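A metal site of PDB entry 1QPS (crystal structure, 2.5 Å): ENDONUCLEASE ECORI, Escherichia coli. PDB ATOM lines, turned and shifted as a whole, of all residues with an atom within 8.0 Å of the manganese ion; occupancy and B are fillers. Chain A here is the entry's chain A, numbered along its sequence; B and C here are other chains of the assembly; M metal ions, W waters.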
ATOM      1  N   VAL A  19     -11.793 -10.569 -22.821  1.00  0.00           N
ATOM      2  CA  VAL A  19     -13.203 -10.912 -23.025  1.00  0.00           C
ATOM      3  C   VAL A  19     -13.432 -11.998 -24.094  1.00  0.00           C
ATOM      4  O   VAL A  19     -14.239 -12.914 -23.891  1.00  0.00           O
ATOM      5  CB  VAL A  19     -14.048  -9.652 -23.369  1.00  0.00           C
ATOM      6  CG1 VAL A  19     -13.666  -9.118 -24.747  1.00  0.00           C
ATOM      7  CG2 VAL A  19     -15.524  -9.972 -23.287  1.00  0.00           C
ATOM      8  N   LYS A  73     -16.763  -8.262 -36.418  1.00  0.00           N
ATOM      9  CA  LYS A  73     -16.124  -9.115 -35.424  1.00  0.00           C
ATOM     10  C   LYS A  73     -16.202  -8.469 -34.032  1.00  0.00           C
ATOM     11  O   LYS A  73     -15.301  -7.725 -33.648  1.00  0.00           O
ATOM     12  CB  LYS A  73     -14.659  -9.362 -35.790  1.00  0.00           C
ATOM     13  CG  LYS A  73     -14.192  -8.692 -37.082  1.00  0.00           C
ATOM     14  CD  LYS A  73     -13.432  -9.669 -37.990  1.00  0.00           C
ATOM     15  CE  LYS A  73     -11.989  -9.898 -37.553  1.00  0.00           C
ATOM     16  NZ  LYS A  73     -11.859 -10.856 -36.412  1.00  0.00           N
ATOM     17  N   PRO A  74     -17.261  -8.710 -33.246  1.00  0.00           N
ATOM     18  CA  PRO A  74     -17.290  -8.243 -31.861  1.00  0.00           C
ATOM     19  C   PRO A  74     -16.119  -8.902 -31.133  1.00  0.00           C
ATOM     20  O   PRO A  74     -15.951 -10.157 -31.252  1.00  0.00           O
ATOM     21  CB  PRO A  74     -18.656  -8.684 -31.371  1.00  0.00           C
ATOM     22  CG  PRO A  74     -19.359  -9.395 -32.521  1.00  0.00           C
ATOM     23  CD  PRO A  74     -18.456  -9.413 -33.716  1.00  0.00           C
ATOM     24  N   ASP A  75     -15.326  -8.091 -30.402  1.00  0.00           N
ATOM     25  CA  ASP A  75     -14.068  -8.579 -29.733  1.00  0.00           C
ATOM     26  C   ASP A  75     -14.320  -9.647 -28.670  1.00  0.00           C
ATOM     27  O   ASP A  75     -13.388 -10.100 -27.983  1.00  0.00           O
ATOM     28  CB  ASP A  75     -13.203  -7.415 -29.133  1.00  0.00           C
ATOM     29  CG  ASP A  75     -13.513  -6.849 -27.689  1.00  0.00           C
ATOM     30  OD1 ASP A  75     -14.299  -7.425 -26.821  1.00  0.00           O
ATOM     31  OD2 ASP A  75     -12.942  -5.762 -27.282  1.00  0.00           O
ATOM     32  N   GLY A  76     -15.565 -10.059 -28.553  1.00  0.00           N
ATOM     33  CA  GLY A  76     -15.963 -11.076 -27.567  1.00  0.00           C
ATOM     34  C   GLY A  76     -16.509 -12.323 -28.266  1.00  0.00           C
ATOM     35  O   GLY A  76     -16.848 -13.327 -27.607  1.00  0.00           O
ATOM     36  N   ALA A  94     -20.427 -10.374 -27.028  1.00  0.00           N
ATOM     37  CA  ALA A  94     -19.855  -9.438 -26.076  1.00  0.00           C
ATOM     38  C   ALA A  94     -18.762  -8.569 -26.694  1.00  0.00           C
ATOM     39  O   ALA A  94     -18.042  -9.004 -27.608  1.00  0.00           O
ATOM     40  CB  ALA A  94     -19.298 -10.181 -24.878  1.00  0.00           C
ATOM     41  N   GLU A  95     -18.659  -7.339 -26.206  1.00  0.00           N
ATOM     42  CA  GLU A  95     -17.610  -6.444 -26.699  1.00  0.00           C
ATOM     43  C   GLU A  95     -17.007  -5.681 -25.529  1.00  0.00           C
ATOM     44  O   GLU A  95     -17.621  -5.455 -24.491  1.00  0.00           O
ATOM     45  CB  GLU A  95     -18.194  -5.466 -27.719  1.00  0.00           C
ATOM     46  CG  GLU A  95     -17.241  -4.316 -28.082  1.00  0.00           C
ATOM     47  CD  GLU A  95     -16.387  -4.585 -29.321  1.00  0.00           C
ATOM     48  OE1 GLU A  95     -15.136  -4.298 -29.324  1.00  0.00           O
ATOM     49  OE2 GLU A  95     -16.888  -5.102 -30.391  1.00  0.00           O
ATOM     50  N   ALA A  96     -15.743  -5.308 -25.710  1.00  0.00           N
ATOM     51  CA  ALA A  96     -15.005  -4.613 -24.667  1.00  0.00           C
ATOM     52  C   ALA A  96     -14.467  -3.278 -25.189  1.00  0.00           C
ATOM     53  O   ALA A  96     -13.877  -3.218 -26.273  1.00  0.00           O
ATOM     54  CB  ALA A  96     -13.878  -5.493 -24.158  1.00  0.00           C
ATOM     55  N   LYS A  97     -14.721  -2.212 -24.441  1.00  0.00           N
ATOM     56  CA  LYS A  97     -14.350  -0.862 -24.851  1.00  0.00           C
ATOM     57  C   LYS A  97     -13.565  -0.142 -23.744  1.00  0.00           C
ATOM     58  O   LYS A  97     -13.791  -0.375 -22.563  1.00  0.00           O
ATOM     59  CB  LYS A  97     -15.597  -0.038 -25.115  1.00  0.00           C
ATOM     60  CG  LYS A  97     -16.505  -0.638 -26.184  1.00  0.00           C
ATOM     61  CD  LYS A  97     -15.963  -0.452 -27.595  1.00  0.00           C
ATOM     62  CE  LYS A  97     -16.868  -1.060 -28.670  1.00  0.00           C
ATOM     63  NZ  LYS A  97     -16.122  -1.615 -29.804  1.00  0.00           N
ATOM     64  N   HIS A  98     -12.578   0.659 -24.148  1.00  0.00           N
ATOM     65  CA  HIS A  98     -11.821   1.475 -23.200  1.00  0.00           C
ATOM     66  C   HIS A  98     -11.958   2.959 -23.538  1.00  0.00           C
ATOM     67  O   HIS A  98     -12.031   3.327 -24.705  1.00  0.00           O
ATOM     68  CB  HIS A  98     -10.342   1.101 -23.238  1.00  0.00           C
ATOM     69  CG  HIS A  98     -10.019  -0.179 -22.525  1.00  0.00           C
ATOM     70  ND1 HIS A  98      -8.734  -0.600 -22.298  1.00  0.00           N
ATOM     71  CD2 HIS A  98     -10.828  -1.138 -21.998  1.00  0.00           C
ATOM     72  CE1 HIS A  98      -8.749  -1.753 -21.656  1.00  0.00           C
ATOM     73  NE2 HIS A  98     -10.010  -2.096 -21.462  1.00  0.00           N
ATOM     74  N   ARG A 129     -19.093   4.741 -31.443  1.00  0.00           N
ATOM     75  CA  ARG A 129     -18.890   3.608 -32.342  1.00  0.00           C
ATOM     76  C   ARG A 129     -19.615   2.347 -31.881  1.00  0.00           C
ATOM     77  O   ARG A 129     -20.228   1.629 -32.673  1.00  0.00           O
ATOM     78  CB  ARG A 129     -17.394   3.283 -32.481  1.00  0.00           C
ATOM     79  CG  ARG A 129     -16.613   4.286 -33.315  1.00  0.00           C
ATOM     80  CD  ARG A 129     -15.587   3.590 -34.183  1.00  0.00           C
ATOM     81  NE  ARG A 129     -14.454   3.104 -33.398  1.00  0.00           N
ATOM     82  CZ  ARG A 129     -14.192   1.820 -33.161  1.00  0.00           C
ATOM     83  NH1 ARG A 129     -13.107   1.483 -32.472  1.00  0.00           N
ATOM     84  NH2 ARG A 129     -14.999   0.864 -33.627  1.00  0.00           N
ATOM     85  N   SER A 130     -19.625   2.144 -30.572  1.00  0.00           N
ATOM     86  CA  SER A 130     -20.240   0.956 -29.973  1.00  0.00           C
ATOM     87  C   SER A 130     -21.672   0.724 -30.429  1.00  0.00           C
ATOM     88  O   SER A 130     -22.163  -0.397 -30.370  1.00  0.00           O
ATOM     89  CB  SER A 130     -20.198   1.058 -28.455  1.00  0.00           C
ATOM     90  OG  SER A 130     -18.940   1.543 -28.019  1.00  0.00           O
ATOM     91  N   ASN A 133     -22.344  -2.030 -34.210  1.00  0.00           N
ATOM     92  CA  ASN A 133     -22.425  -3.458 -33.905  1.00  0.00           C
ATOM     93  C   ASN A 133     -23.692  -3.837 -33.118  1.00  0.00           C
ATOM     94  O   ASN A 133     -24.332  -4.838 -33.428  1.00  0.00           O
ATOM     95  CB  ASN A 133     -21.190  -3.899 -33.113  1.00  0.00           C
ATOM     96  CG  ASN A 133     -19.972  -4.131 -34.008  1.00  0.00           C
ATOM     97  OD1 ASN A 133     -19.982  -3.807 -35.188  1.00  0.00           O
ATOM     98  ND2 ASN A 133     -18.907  -4.676 -33.413  1.00  0.00           N
ATOM     99  N   LEU A 151     -21.895  -5.253 -23.273  1.00  0.00           N
ATOM    100  CA  LEU A 151     -20.797  -4.326 -23.524  1.00  0.00           C
ATOM    101  C   LEU A 151     -20.089  -3.984 -22.215  1.00  0.00           C
ATOM    102  O   LEU A 151     -20.734  -3.617 -21.234  1.00  0.00           O
ATOM    103  CB  LEU A 151     -21.330  -3.058 -24.201  1.00  0.00           C
ATOM    104  CG  LEU A 151     -20.344  -1.920 -24.509  1.00  0.00           C
ATOM    105  CD1 LEU A 151     -19.179  -2.434 -25.329  1.00  0.00           C
ATOM    106  CD2 LEU A 151     -21.075  -0.828 -25.252  1.00  0.00           C
ATOM    107  N   PHE A 152     -18.783  -4.220 -22.177  1.00  0.00           N
ATOM    108  CA  PHE A 152     -17.973  -3.988 -20.986  1.00  0.00           C
ATOM    109  C   PHE A 152     -17.131  -2.715 -21.104  1.00  0.00           C
ATOM    110  O   PHE A 152     -16.312  -2.569 -22.025  1.00  0.00           O
ATOM    111  CB  PHE A 152     -17.041  -5.182 -20.731  1.00  0.00           C
ATOM    112  CG  PHE A 152     -17.739  -6.376 -20.167  1.00  0.00           C
ATOM    113  CD1 PHE A 152     -18.005  -7.484 -20.961  1.00  0.00           C
ATOM    114  CD2 PHE A 152     -18.134  -6.400 -18.826  1.00  0.00           C
ATOM    115  CE1 PHE A 152     -18.662  -8.590 -20.431  1.00  0.00           C
ATOM    116  CE2 PHE A 152     -18.786  -7.509 -18.309  1.00  0.00           C
ATOM    117  CZ  PHE A 152     -19.052  -8.603 -19.105  1.00  0.00           C
ATOM    118  OP3  DA B   1     -12.308  -2.229 -31.327  1.00  0.00           O
ATOM    119  P    DA B   1     -12.736  -1.267 -30.274  1.00  0.00           P
ATOM    120  OP1  DA B   1     -13.854  -0.533 -30.935  1.00  0.00           O
ATOM    121  OP2  DA B   1     -12.982  -1.971 -28.983  1.00  0.00           O
ATOM    122  O5'  DA B   1     -11.531  -0.293 -30.089  1.00  0.00           O
ATOM    123  C5'  DA B   1     -10.281  -0.875 -29.697  1.00  0.00           C
ATOM    124  C4'  DA B   1      -9.037  -0.364 -30.374  1.00  0.00           C
ATOM    125  O4'  DA B   1      -9.266  -0.036 -31.734  1.00  0.00           O
ATOM    126  C3'  DA B   1      -8.618   0.917 -29.719  1.00  0.00           C
ATOM    127  O3'  DA B   1      -7.634   0.593 -28.711  1.00  0.00           O
ATOM    128  C2'  DA B   1      -7.993   1.701 -30.890  1.00  0.00           C
ATOM    129  C1'  DA B   1      -8.313   0.943 -32.141  1.00  0.00           C
ATOM    130  N9   DA B   1      -8.991   1.717 -33.132  1.00  0.00           N
ATOM    131  C8   DA B   1     -10.316   1.741 -33.425  1.00  0.00           C
ATOM    132  N7   DA B   1     -10.629   2.369 -34.510  1.00  0.00           N
ATOM    133  C5   DA B   1      -9.385   2.807 -34.966  1.00  0.00           C
ATOM    134  C6   DA B   1      -8.967   3.529 -36.100  1.00  0.00           C
ATOM    135  N6   DA B   1      -9.800   4.014 -37.005  1.00  0.00           N
ATOM    136  N1   DA B   1      -7.669   3.777 -36.263  1.00  0.00           N
ATOM    137  C2   DA B   1      -6.829   3.326 -35.329  1.00  0.00           C
ATOM    138  N3   DA B   1      -7.073   2.650 -34.228  1.00  0.00           N
ATOM    139  C4   DA B   1      -8.386   2.416 -34.112  1.00  0.00           C
ATOM    140  P    DA B   2      -7.830   0.926 -27.160  1.00  0.00           P
ATOM    141  OP1  DA B   2      -6.694   0.710 -26.250  1.00  0.00           O
ATOM    142  OP2  DA B   2      -9.196   0.554 -26.735  1.00  0.00           O
ATOM    143  O5'  DA B   2      -8.572   2.297 -27.538  1.00  0.00           O
ATOM    144  C5'  DA B   2      -7.708   3.411 -27.576  1.00  0.00           C
ATOM    145  C4'  DA B   2      -8.360   4.729 -27.977  1.00  0.00           C
ATOM    146  O4'  DA B   2      -8.999   4.605 -29.127  1.00  0.00           O
ATOM    147  C3'  DA B   2      -9.328   5.302 -27.120  1.00  0.00           C
ATOM    148  O3'  DA B   2      -8.384   5.944 -26.431  1.00  0.00           O
ATOM    149  C2'  DA B   2     -10.605   5.583 -28.015  1.00  0.00           C
ATOM    150  C1'  DA B   2      -9.936   5.625 -29.443  1.00  0.00           C
ATOM    151  N9   DA B   2     -10.654   5.325 -30.709  1.00  0.00           N
ATOM    152  C8   DA B   2     -11.577   4.370 -30.977  1.00  0.00           C
ATOM    153  N7   DA B   2     -12.027   4.372 -32.212  1.00  0.00           N
ATOM    154  C5   DA B   2     -11.336   5.435 -32.790  1.00  0.00           C
ATOM    155  C6   DA B   2     -11.357   5.994 -34.065  1.00  0.00           C
ATOM    156  N6   DA B   2     -12.138   5.569 -35.028  1.00  0.00           N
ATOM    157  N1   DA B   2     -10.576   7.039 -34.307  1.00  0.00           N
ATOM    158  C2   DA B   2      -9.810   7.480 -33.337  1.00  0.00           C
ATOM    159  N3   DA B   2      -9.692   7.036 -32.108  1.00  0.00           N
ATOM    160  C4   DA B   2     -10.504   6.000 -31.896  1.00  0.00           C
ATOM    161  P    DG C   5     -16.008  -4.367 -37.156  1.00  0.00           P
ATOM    162  OP1  DG C   5     -16.931  -5.116 -36.289  1.00  0.00           O
ATOM    163  OP2  DG C   5     -16.596  -3.261 -37.956  1.00  0.00           O
ATOM    164  O5'  DG C   5     -14.793  -3.784 -36.271  1.00  0.00           O
ATOM    165  C5'  DG C   5     -14.110  -4.665 -35.324  1.00  0.00           C
ATOM    166  C4'  DG C   5     -12.904  -3.917 -34.708  1.00  0.00           C
ATOM    167  O4'  DG C   5     -11.766  -3.762 -35.587  1.00  0.00           O
ATOM    168  C3'  DG C   5     -13.343  -2.477 -34.524  1.00  0.00           C
ATOM    169  O3'  DG C   5     -14.232  -2.348 -33.356  1.00  0.00           O
ATOM    170  C2'  DG C   5     -11.992  -1.820 -34.369  1.00  0.00           C
ATOM    171  C1'  DG C   5     -11.098  -2.530 -35.362  1.00  0.00           C
ATOM    172  N9   DG C   5     -11.010  -1.704 -36.583  1.00  0.00           N
ATOM    173  C8   DG C   5     -11.964  -1.478 -37.540  1.00  0.00           C
ATOM    174  N7   DG C   5     -11.590  -0.623 -38.464  1.00  0.00           N
ATOM    175  C5   DG C   5     -10.297  -0.276 -38.086  1.00  0.00           C
ATOM    176  C6   DG C   5      -9.383   0.613 -38.697  1.00  0.00           C
ATOM    177  O6   DG C   5      -9.521   1.296 -39.715  1.00  0.00           O
ATOM    178  N1   DG C   5      -8.193   0.666 -37.992  1.00  0.00           N
ATOM    179  C2   DG C   5      -7.917  -0.034 -36.858  1.00  0.00           C
ATOM    180  N2   DG C   5      -6.755   0.169 -36.296  1.00  0.00           N
ATOM    181  N3   DG C   5      -8.770  -0.869 -36.275  1.00  0.00           N
ATOM    182  C4   DG C   5      -9.940  -0.938 -36.946  1.00  0.00           C
HETATM  183 MN    MN M   1     -13.158  -3.877 -28.390  1.00  0.00          MN
HETATM  184  O   HOH W   1     -12.478  -4.820 -30.309  1.00  0.00           O
HETATM  185  O   HOH W   2     -11.280  -3.346 -27.523  1.00  0.00           O
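OP1 of DA 1 of chain B is in salt-bridge range of NZ of Lys 97 (2.8 Å).
The guanidinium group (NH1) of Arg 129 lies within salt-bridge range of OP1 of DA 1 of chain B, at 2.6 Å.
The side-chain carboxylate of Glu 95 is in salt-bridge range of the side-chain amino group of Lys 97.
The backbone NH (N) of Phe 152 lies within hydrogen-bond range of the backbone carbonyl oxygen (O) of Glu 95.
N of Lys 97 lies within hydrogen-bond range of O of Phe 152, at 2.9 Å.
Merely in contact with the manganese ion: Lys 97 (3.99 Å).
The nearest printed residue that does not touch the manganese ion is DG 5 of chain C (5.3 Å).
OP2 of DA 1 of chain B binds the manganese ion (2.0 Å).
The manganese ion is bound by water W2 (2.1 Å).
The side-chain carboxylate (OD2) of Asp 75 binds the manganese ion (2.2 Å).
OE1 of Glu 95 binds the manganese ion (2.2 Å).
Water W1 binds the manganese ion (2.2 Å).
The manganese ion is bound by O of Ala 96 (2.3 Å).
The manganese ion has six donor atoms within binding distance.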
